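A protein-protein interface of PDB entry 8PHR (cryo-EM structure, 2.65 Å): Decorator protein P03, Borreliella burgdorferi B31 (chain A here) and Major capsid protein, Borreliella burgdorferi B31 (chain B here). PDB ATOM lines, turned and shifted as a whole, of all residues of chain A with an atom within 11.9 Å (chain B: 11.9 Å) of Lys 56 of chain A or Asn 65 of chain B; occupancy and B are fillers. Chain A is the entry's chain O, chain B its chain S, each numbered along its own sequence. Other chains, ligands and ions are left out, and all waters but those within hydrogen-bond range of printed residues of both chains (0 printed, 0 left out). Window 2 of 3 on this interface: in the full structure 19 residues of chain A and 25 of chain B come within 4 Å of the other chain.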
ATOM      1  N   GLY A  50      13.558  11.499  18.028  1.00  0.00           N
ATOM      2  CA  GLY A  50      13.049  12.708  17.426  1.00  0.00           C
ATOM      3  C   GLY A  50      13.817  13.923  17.907  1.00  0.00           C
ATOM      4  O   GLY A  50      14.441  13.917  18.968  1.00  0.00           O
ATOM      5  N   VAL A  51      13.762  14.979  17.092  1.00  0.00           N
ATOM      6  CA  VAL A  51      14.428  16.226  17.452  1.00  0.00           C
ATOM      7  C   VAL A  51      13.750  16.867  18.657  1.00  0.00           C
ATOM      8  O   VAL A  51      14.417  17.416  19.542  1.00  0.00           O
ATOM      9  CB  VAL A  51      14.473  17.178  16.243  1.00  0.00           C
ATOM     10  CG1 VAL A  51      15.471  16.673  15.213  1.00  0.00           C
ATOM     11  CG2 VAL A  51      13.094  17.317  15.615  1.00  0.00           C
ATOM     12  N   CYS A  52      12.422  16.811  18.711  1.00  0.00           N
ATOM     13  CA  CYS A  52      11.644  17.322  19.836  1.00  0.00           C
ATOM     14  C   CYS A  52      10.815  16.171  20.392  1.00  0.00           C
ATOM     15  O   CYS A  52       9.874  15.707  19.741  1.00  0.00           O
ATOM     16  CB  CYS A  52      10.756  18.488  19.407  1.00  0.00           C
ATOM     17  SG  CYS A  52      11.659  19.978  18.924  1.00  0.00           S
ATOM     18  N   THR A  53      11.163  15.715  21.593  1.00  0.00           N
ATOM     19  CA  THR A  53      10.522  14.566  22.218  1.00  0.00           C
ATOM     20  C   THR A  53       9.897  14.990  23.540  1.00  0.00           C
ATOM     21  O   THR A  53      10.534  15.684  24.339  1.00  0.00           O
ATOM     22  CB  THR A  53      11.527  13.432  22.447  1.00  0.00           C
ATOM     23  OG1 THR A  53      12.081  13.021  21.191  1.00  0.00           O
ATOM     24  CG2 THR A  53      10.851  12.241  23.110  1.00  0.00           C
ATOM     25  N   SER A  54       8.655  14.573  23.762  1.00  0.00           N
ATOM     26  CA  SER A  54       7.931  14.865  24.989  1.00  0.00           C
ATOM     27  C   SER A  54       7.989  13.671  25.936  1.00  0.00           C
ATOM     28  O   SER A  54       8.072  12.518  25.508  1.00  0.00           O
ATOM     29  CB  SER A  54       6.473  15.220  24.692  1.00  0.00           C
ATOM     30  OG  SER A  54       5.731  15.368  25.890  1.00  0.00           O
ATOM     31  N   SER A  55       7.948  13.966  27.236  1.00  0.00           N
ATOM     32  CA  SER A  55       7.978  12.919  28.249  1.00  0.00           C
ATOM     33  C   SER A  55       6.668  12.149  28.347  1.00  0.00           C
ATOM     34  O   SER A  55       6.626  11.124  29.035  1.00  0.00           O
ATOM     35  CB  SER A  55       8.326  13.520  29.613  1.00  0.00           C
ATOM     36  OG  SER A  55       7.412  14.545  29.965  1.00  0.00           O
ATOM     37  N   LYS A  56       5.611  12.610  27.682  1.00  0.00           N
ATOM     38  CA  LYS A  56       4.306  11.958  27.704  1.00  0.00           C
ATOM     39  C   LYS A  56       3.998  11.286  26.369  1.00  0.00           C
ATOM     40  O   LYS A  56       2.852  11.262  25.917  1.00  0.00           O
ATOM     41  CB  LYS A  56       3.208  12.957  28.062  1.00  0.00           C
ATOM     42  CG  LYS A  56       3.498  13.792  29.300  1.00  0.00           C
ATOM     43  CD  LYS A  56       3.824  12.920  30.502  1.00  0.00           C
ATOM     44  CE  LYS A  56       4.481  13.732  31.606  1.00  0.00           C
ATOM     45  NZ  LYS A  56       3.672  14.926  31.971  1.00  0.00           N
ATOM     46  N   ASP A  57       5.020  10.730  25.725  1.00  0.00           N
ATOM     47  CA  ASP A  57       4.855  10.071  24.438  1.00  0.00           C
ATOM     48  C   ASP A  57       4.637   8.576  24.630  1.00  0.00           C
ATOM     49  O   ASP A  57       5.254   7.952  25.496  1.00  0.00           O
ATOM     50  CB  ASP A  57       6.075  10.311  23.548  1.00  0.00           C
ATOM     51  CG  ASP A  57       6.091  11.700  22.942  1.00  0.00           C
ATOM     52  OD1 ASP A  57       4.999  12.262  22.715  1.00  0.00           O
ATOM     53  OD2 ASP A  57       7.195  12.228  22.692  1.00  0.00           O
ATOM     54  N   LYS A  58       3.753   8.008  23.813  1.00  0.00           N
ATOM     55  CA  LYS A  58       3.451   6.583  23.863  1.00  0.00           C
ATOM     56  C   LYS A  58       4.337   5.850  22.861  1.00  0.00           C
ATOM     57  O   LYS A  58       4.293   6.135  21.659  1.00  0.00           O
ATOM     58  CB  LYS A  58       1.973   6.333  23.568  1.00  0.00           C
ATOM     59  CG  LYS A  58       1.587   4.865  23.546  1.00  0.00           C
ATOM     60  CD  LYS A  58       0.090   4.692  23.737  1.00  0.00           C
ATOM     61  CE  LYS A  58      -0.339   3.261  23.466  1.00  0.00           C
ATOM     62  NZ  LYS A  58       0.616   2.268  24.022  1.00  0.00           N
ATOM     63  N   ILE A  59       5.139   4.912  23.360  1.00  0.00           N
ATOM     64  CA  ILE A  59       6.133   4.200  22.566  1.00  0.00           C
ATOM     65  C   ILE A  59       5.878   2.705  22.687  1.00  0.00           C
ATOM     66  O   ILE A  59       5.723   2.187  23.799  1.00  0.00           O
ATOM     67  CB  ILE A  59       7.563   4.546  23.018  1.00  0.00           C
ATOM     68  CG1 ILE A  59       7.785   6.061  22.990  1.00  0.00           C
ATOM     69  CG2 ILE A  59       8.581   3.828  22.162  1.00  0.00           C
ATOM     70  CD1 ILE A  59       9.132   6.490  23.528  1.00  0.00           C
ATOM     71  N   GLU A  60       5.830   2.016  21.551  1.00  0.00           N
ATOM     72  CA  GLU A  60       5.649   0.574  21.510  1.00  0.00           C
ATOM     73  C   GLU A  60       6.866  -0.085  20.872  1.00  0.00           C
ATOM     74  O   GLU A  60       7.700   0.571  20.246  1.00  0.00           O
ATOM     75  CB  GLU A  60       4.377   0.212  20.736  1.00  0.00           C
ATOM     76  CG  GLU A  60       3.102   0.762  21.352  1.00  0.00           C
ATOM     77  CD  GLU A  60       1.939   0.768  20.382  1.00  0.00           C
ATOM     78  OE1 GLU A  60       2.152   0.461  19.191  1.00  0.00           O
ATOM     79  OE2 GLU A  60       0.809   1.082  20.811  1.00  0.00           O
ATOM     80  N   VAL A 110       8.130   1.856  17.719  1.00  0.00           N
ATOM     81  CA  VAL A 110       7.039   2.417  16.935  1.00  0.00           C
ATOM     82  C   VAL A 110       6.341   3.498  17.747  1.00  0.00           C
ATOM     83  O   VAL A 110       6.050   3.315  18.936  1.00  0.00           O
ATOM     84  CB  VAL A 110       6.034   1.326  16.501  1.00  0.00           C
ATOM     85  CG1 VAL A 110       4.804   1.950  15.857  1.00  0.00           C
ATOM     86  CG2 VAL A 110       6.697   0.342  15.548  1.00  0.00           C
ATOM     87  N   ILE A 111       6.091   4.631  17.104  1.00  0.00           N
ATOM     88  CA  ILE A 111       5.238   5.693  17.628  1.00  0.00           C
ATOM     89  C   ILE A 111       3.935   5.659  16.838  1.00  0.00           C
ATOM     90  O   ILE A 111       3.955   5.878  15.619  1.00  0.00           O
ATOM     91  CB  ILE A 111       5.913   7.069  17.530  1.00  0.00           C
ATOM     92  CG1 ILE A 111       7.220   7.074  18.327  1.00  0.00           C
ATOM     93  CG2 ILE A 111       4.976   8.160  18.024  1.00  0.00           C
ATOM     94  CD1 ILE A 111       7.934   8.404  18.326  1.00  0.00           C
ATOM     95  N   PRO A 112       2.796   5.378  17.471  1.00  0.00           N
ATOM     96  CA  PRO A 112       1.553   5.208  16.712  1.00  0.00           C
ATOM     97  C   PRO A 112       1.144   6.485  15.996  1.00  0.00           C
ATOM     98  O   PRO A 112       1.479   7.596  16.415  1.00  0.00           O
ATOM     99  CB  PRO A 112       0.530   4.817  17.787  1.00  0.00           C
ATOM    100  CG  PRO A 112       1.352   4.326  18.942  1.00  0.00           C
ATOM    101  CD  PRO A 112       2.601   5.147  18.911  1.00  0.00           C
ATOM    102  N   THR A 114      -1.586   7.804  15.984  1.00  0.00           N
ATOM    103  CA  THR A 114      -2.417   8.610  16.868  1.00  0.00           C
ATOM    104  C   THR A 114      -1.606   9.610  17.681  1.00  0.00           C
ATOM    105  O   THR A 114      -2.191  10.542  18.244  1.00  0.00           O
ATOM    106  CB  THR A 114      -3.207   7.704  17.812  1.00  0.00           C
ATOM    107  OG1 THR A 114      -2.308   7.065  18.727  1.00  0.00           O
ATOM    108  CG2 THR A 114      -3.961   6.643  17.026  1.00  0.00           C
ATOM    109  N   ASN A 115      -0.289   9.443  17.753  1.00  0.00           N
ATOM    110  CA  ASN A 115       0.593  10.352  18.471  1.00  0.00           C
ATOM    111  C   ASN A 115       1.479  11.072  17.465  1.00  0.00           C
ATOM    112  O   ASN A 115       2.108  10.432  16.617  1.00  0.00           O
ATOM    113  CB  ASN A 115       1.444   9.592  19.491  1.00  0.00           C
ATOM    114  CG  ASN A 115       2.184  10.515  20.443  1.00  0.00           C
ATOM    115  OD1 ASN A 115       2.163  11.736  20.288  1.00  0.00           O
ATOM    116  ND2 ASN A 115       2.846   9.931  21.434  1.00  0.00           N
ATOM    117  N   ASN A 116       1.521  12.399  17.558  1.00  0.00           N
ATOM    118  CA  ASN A 116       2.295  13.190  16.613  1.00  0.00           C
ATOM    119  C   ASN A 116       3.792  12.987  16.829  1.00  0.00           C
ATOM    120  O   ASN A 116       4.259  12.758  17.948  1.00  0.00           O
ATOM    121  CB  ASN A 116       1.938  14.671  16.737  1.00  0.00           C
ATOM    122  CG  ASN A 116       2.603  15.333  17.924  1.00  0.00           C
ATOM    123  OD1 ASN A 116       2.442  14.893  19.061  1.00  0.00           O
ATOM    124  ND2 ASN A 116       3.352  16.399  17.667  1.00  0.00           N
ATOM    125  N   PHE A 117       4.545  13.067  15.733  1.00  0.00           N
ATOM    126  CA  PHE A 117       5.985  12.853  15.759  1.00  0.00           C
ATOM    127  C   PHE A 117       6.677  13.891  14.889  1.00  0.00           C
ATOM    128  O   PHE A 117       6.164  14.271  13.834  1.00  0.00           O
ATOM    129  CB  PHE A 117       6.349  11.442  15.277  1.00  0.00           C
ATOM    130  CG  PHE A 117       7.822  11.232  15.067  1.00  0.00           C
ATOM    131  CD1 PHE A 117       8.676  11.094  16.148  1.00  0.00           C
ATOM    132  CD2 PHE A 117       8.352  11.173  13.788  1.00  0.00           C
ATOM    133  CE1 PHE A 117      10.031  10.900  15.959  1.00  0.00           C
ATOM    134  CE2 PHE A 117       9.707  10.981  13.593  1.00  0.00           C
ATOM    135  CZ  PHE A 117      10.547  10.844  14.679  1.00  0.00           C
ATOM    136  N   THR A 118       7.845  14.344  15.342  1.00  0.00           N
ATOM    137  CA  THR A 118       8.684  15.271  14.591  1.00  0.00           C
ATOM    138  C   THR A 118      10.103  14.727  14.572  1.00  0.00           C
ATOM    139  O   THR A 118      10.707  14.529  15.632  1.00  0.00           O
ATOM    140  CB  THR A 118       8.655  16.673  15.206  1.00  0.00           C
ATOM    141  OG1 THR A 118       7.301  17.139  15.280  1.00  0.00           O
ATOM    142  CG2 THR A 118       9.479  17.640  14.369  1.00  0.00           C
ATOM    143  N   ASN B  56      16.943  23.887  17.849  1.00  0.00           N
ATOM    144  CA  ASN B  56      17.141  25.063  18.677  1.00  0.00           C
ATOM    145  C   ASN B  56      16.623  24.807  20.093  1.00  0.00           C
ATOM    146  O   ASN B  56      15.733  23.978  20.295  1.00  0.00           O
ATOM    147  CB  ASN B  56      16.427  26.267  18.068  1.00  0.00           C
ATOM    148  CG  ASN B  56      16.854  26.536  16.640  1.00  0.00           C
ATOM    149  OD1 ASN B  56      18.045  26.643  16.345  1.00  0.00           O
ATOM    150  ND2 ASN B  56      15.882  26.646  15.741  1.00  0.00           N
ATOM    151  N   PRO B  57      17.171  25.502  21.091  1.00  0.00           N
ATOM    152  CA  PRO B  57      16.729  25.277  22.472  1.00  0.00           C
ATOM    153  C   PRO B  57      15.268  25.659  22.663  1.00  0.00           C
ATOM    154  O   PRO B  57      14.696  26.450  21.910  1.00  0.00           O
ATOM    155  CB  PRO B  57      17.653  26.182  23.297  1.00  0.00           C
ATOM    156  CG  PRO B  57      18.818  26.466  22.407  1.00  0.00           C
ATOM    157  CD  PRO B  57      18.273  26.476  21.017  1.00  0.00           C
ATOM    158  N   THR B  58      14.665  25.074  23.692  1.00  0.00           N
ATOM    159  CA  THR B  58      13.253  25.264  23.990  1.00  0.00           C
ATOM    160  C   THR B  58      13.095  26.315  25.082  1.00  0.00           C
ATOM    161  O   THR B  58      13.760  26.243  26.122  1.00  0.00           O
ATOM    162  CB  THR B  58      12.609  23.946  24.428  1.00  0.00           C
ATOM    163  OG1 THR B  58      12.590  23.033  23.323  1.00  0.00           O
ATOM    164  CG2 THR B  58      11.187  24.176  24.912  1.00  0.00           C
ATOM    165  N   THR B  59      12.218  27.287  24.842  1.00  0.00           N
ATOM    166  CA  THR B  59      11.942  28.329  25.824  1.00  0.00           C
ATOM    167  C   THR B  59      11.060  27.760  26.929  1.00  0.00           C
ATOM    168  O   THR B  59       9.976  27.234  26.655  1.00  0.00           O
ATOM    169  CB  THR B  59      11.265  29.526  25.160  1.00  0.00           C
ATOM    170  OG1 THR B  59      12.075  29.998  24.076  1.00  0.00           O
ATOM    171  CG2 THR B  59      11.068  30.652  26.167  1.00  0.00           C
ATOM    172  N   ILE B  60      11.524  27.863  28.172  1.00  0.00           N
ATOM    173  CA  ILE B  60      10.786  27.337  29.322  1.00  0.00           C
ATOM    174  C   ILE B  60       9.867  28.460  29.797  1.00  0.00           C
ATOM    175  O   ILE B  60      10.205  29.244  30.684  1.00  0.00           O
ATOM    176  CB  ILE B  60      11.718  26.836  30.422  1.00  0.00           C
ATOM    177  CG1 ILE B  60      12.645  25.756  29.867  1.00  0.00           C
ATOM    178  CG2 ILE B  60      10.918  26.280  31.590  1.00  0.00           C
ATOM    179  CD1 ILE B  60      11.906  24.575  29.276  1.00  0.00           C
ATOM    180  N   ALA B  61       8.687  28.535  29.188  1.00  0.00           N
ATOM    181  CA  ALA B  61       7.673  29.512  29.555  1.00  0.00           C
ATOM    182  C   ALA B  61       6.363  28.784  29.808  1.00  0.00           C
ATOM    183  O   ALA B  61       5.918  27.994  28.968  1.00  0.00           O
ATOM    184  CB  ALA B  61       7.493  30.568  28.461  1.00  0.00           C
ATOM    185  N   ASN B  62       5.758  29.044  30.965  1.00  0.00           N
ATOM    186  CA  ASN B  62       4.466  28.464  31.356  1.00  0.00           C
ATOM    187  C   ASN B  62       4.652  26.949  31.438  1.00  0.00           C
ATOM    188  O   ASN B  62       5.636  26.494  32.042  1.00  0.00           O
ATOM    189  CB  ASN B  62       3.388  28.952  30.398  1.00  0.00           C
ATOM    190  CG  ASN B  62       3.097  30.432  30.557  1.00  0.00           C
ATOM    191  OD1 ASN B  62       2.319  31.008  29.798  1.00  0.00           O
ATOM    192  ND2 ASN B  62       3.715  31.053  31.554  1.00  0.00           N
ATOM    193  N   GLU B  63       3.761  26.146  30.865  1.00  0.00           N
ATOM    194  CA  GLU B  63       3.872  24.694  30.892  1.00  0.00           C
ATOM    195  C   GLU B  63       4.273  24.195  29.512  1.00  0.00           C
ATOM    196  O   GLU B  63       3.745  24.668  28.500  1.00  0.00           O
ATOM    197  CB  GLU B  63       2.554  24.046  31.322  1.00  0.00           C
ATOM    198  CG  GLU B  63       1.979  24.593  32.618  1.00  0.00           C
ATOM    199  CD  GLU B  63       0.638  23.975  32.964  1.00  0.00           C
ATOM    200  OE1 GLU B  63       0.159  23.120  32.189  1.00  0.00           O
ATOM    201  OE2 GLU B  63       0.063  24.344  34.008  1.00  0.00           O
ATOM    202  N   VAL B  64       5.210  23.253  29.472  1.00  0.00           N
ATOM    203  CA  VAL B  64       5.647  22.650  28.218  1.00  0.00           C
ATOM    204  C   VAL B  64       6.139  21.239  28.511  1.00  0.00           C
ATOM    205  O   VAL B  64       6.734  20.979  29.561  1.00  0.00           O
ATOM    206  CB  VAL B  64       6.732  23.507  27.526  1.00  0.00           C
ATOM    207  CG1 VAL B  64       7.992  23.577  28.375  1.00  0.00           C
ATOM    208  CG2 VAL B  64       7.041  22.964  26.139  1.00  0.00           C
ATOM    209  N   ASN B  65       5.865  20.323  27.586  1.00  0.00           N
ATOM    210  CA  ASN B  65       6.308  18.941  27.702  1.00  0.00           C
ATOM    211  C   ASN B  65       7.277  18.515  26.610  1.00  0.00           C
ATOM    212  O   ASN B  65       8.124  17.655  26.861  1.00  0.00           O
ATOM    213  CB  ASN B  65       5.101  17.990  27.693  1.00  0.00           C
ATOM    214  CG  ASN B  65       4.396  17.932  29.034  1.00  0.00           C
ATOM    215  OD1 ASN B  65       4.920  18.399  30.045  1.00  0.00           O
ATOM    216  ND2 ASN B  65       3.197  17.359  29.047  1.00  0.00           N
ATOM    217  N   THR B  66       7.179  19.089  25.415  1.00  0.00           N
ATOM    218  CA  THR B  66       8.061  18.740  24.308  1.00  0.00           C
ATOM    219  C   THR B  66       9.298  19.630  24.352  1.00  0.00           C
ATOM    220  O   THR B  66       9.194  20.855  24.220  1.00  0.00           O
ATOM    221  CB  THR B  66       7.335  18.892  22.972  1.00  0.00           C
ATOM    222  OG1 THR B  66       6.036  18.295  23.064  1.00  0.00           O
ATOM    223  CG2 THR B  66       8.118  18.210  21.864  1.00  0.00           C
ATOM    224  N   ILE B  67      10.464  19.016  24.537  1.00  0.00           N
ATOM    225  CA  ILE B  67      11.727  19.733  24.651  1.00  0.00           C
ATOM    226  C   ILE B  67      12.676  19.230  23.573  1.00  0.00           C
ATOM    227  O   ILE B  67      12.640  18.060  23.182  1.00  0.00           O
ATOM    228  CB  ILE B  67      12.355  19.570  26.053  1.00  0.00           C
ATOM    229  CG1 ILE B  67      11.289  19.710  27.141  1.00  0.00           C
ATOM    230  CG2 ILE B  67      13.462  20.592  26.271  1.00  0.00           C
ATOM    231  CD1 ILE B  67      10.681  21.093  27.227  1.00  0.00           C
ATOM    232  N   SER B  68      13.528  20.131  23.088  1.00  0.00           N
ATOM    233  CA  SER B  68      14.539  19.758  22.109  1.00  0.00           C
ATOM    234  C   SER B  68      15.544  18.791  22.726  1.00  0.00           C
ATOM    235  O   SER B  68      15.839  18.844  23.922  1.00  0.00           O
ATOM    236  CB  SER B  68      15.258  21.000  21.582  1.00  0.00           C
ATOM    237  OG  SER B  68      14.381  21.817  20.827  1.00  0.00           O
ATOM    238  N   THR B  69      16.074  17.903  21.891  1.00  0.00           N
ATOM    239  CA  THR B  69      16.933  16.823  22.347  1.00  0.00           C
ATOM    240  C   THR B  69      18.368  17.030  21.875  1.00  0.00           C
ATOM    241  O   THR B  69      18.631  17.699  20.872  1.00  0.00           O
ATOM    242  CB  THR B  69      16.422  15.466  21.851  1.00  0.00           C
ATOM    243  OG1 THR B  69      16.134  15.544  20.448  1.00  0.00           O
ATOM    244  CG2 THR B  69      15.161  15.064  22.602  1.00  0.00           C
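OG of Ser 68 of chain B sits at hydrogen-bond distance from SG of Cys 52 of chain A (3.8 Å).
The side-chain hydroxyl of Thr 69 of chain B sits at hydrogen-bond distance from the backbone carbonyl oxygen of Gly 50 of chain A (2.8 Å).
The backbone carbonyl oxygen (O) of Asn 65 of chain B lies close to the side-chain hydroxyl (OG) of Ser 54 of chain A, at 3.4 Å.
The side-chain hydroxyl (OG1) of Thr 69 of chain B sits at hydrogen-bond distance from the backbone carbonyl oxygen (O) of Val 51 of chain A (2.7 Å).
The backbone carbonyl oxygen (O) of Ile 67 of chain B lies within hydrogen-bond range of the backbone NH (N) of Thr 53 of chain A (3.2 Å).
N of Ser 68 of chain B lies within hydrogen-bond range of OG1 of Thr 58 of chain B (3.1 Å).
The backbone NH (N) of Val 51 of chain A is in hydrogen-bond range of the backbone carbonyl oxygen (O) of Thr 118 of chain A.
The side-chain hydroxyl (OG) of Ser 68 of chain B sits at hydrogen-bond distance from the backbone carbonyl oxygen (O) of Asn 56 of chain B, at 2.6 Å.
The backbone carbonyl oxygen of Gly 50 of chain A is in hydrogen-bond range of the side-chain hydroxyl of Thr 53 of chain A, at 3.4 Å.
OG of Ser 54 of chain A lies close to N of Lys 56 of chain A.
N of Ser 54 of chain A lies within hydrogen-bond range of OD2 of Asp 57 of chain A (3.0 Å).
O of Val 51 of chain A touches CA of Ser 68 of chain B, 3.5 Å away.
Cys 52 of chain A touches Thr 66 of chain B.
Ile 67 of chain B touches Cys 52 of chain A (O to CA, 3.6 Å).
Thr 66 of chain B touches Thr 53 of chain A.
OG1 of Thr 53 of chain A touches CG2 of Thr 69 of chain B, at 3.96 Å.
Thr 66 of chain B touches Ser 54 of chain A (OG1 to CB, 3.5 Å).
Asn 65 of chain B touches Ser 55 of chain A (O to N, 3.7 Å).
Lys 56 of chain A touches Asn 65 of chain B (CG to ND2, 3.6 Å).
Of the printed residues of chain B, Val 51 of chain A touches Ser 68 (3.5 Å) and Thr 69 (2.7 Å).
Printed residues of chain B within 4 Å of Cys 52 of chain A: Thr 66, Ile 67 and Ser 68.
Of the printed residues of chain B, Thr 53 of chain A touches Thr 66 (3.9 Å), Ile 67 (3.2 Å) and Thr 69 (3.96 Å).
Ser 54 of chain A touches just these residues of chain B: Asn 65 (3.2 Å) and Thr 66 (3.5 Å).
Ser 55 of chain A touches just one residue of chain B: Asn 65 (3.7 Å).
Lys 56 of chain A touches just one residue of chain B: Asn 65 (3.6 Å).
No residue of chain B comes within 4 Å of Asp 57 of chain A.
Printed residues of chain A within 4 Å of Ile 67 of chain B: Cys 52 and Thr 53.
Printed residues of chain A within 4 Å of Ser 68 of chain B: Val 51 (3.5 Å) and Cys 52 (3.8 Å).
Among the printed residues, 13 pairs touch across the chains.
Among the printed residues, no Asp or Glu carboxylate lies within 4 Å of a Lys or Arg side-chain nitrogen of the other chain.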
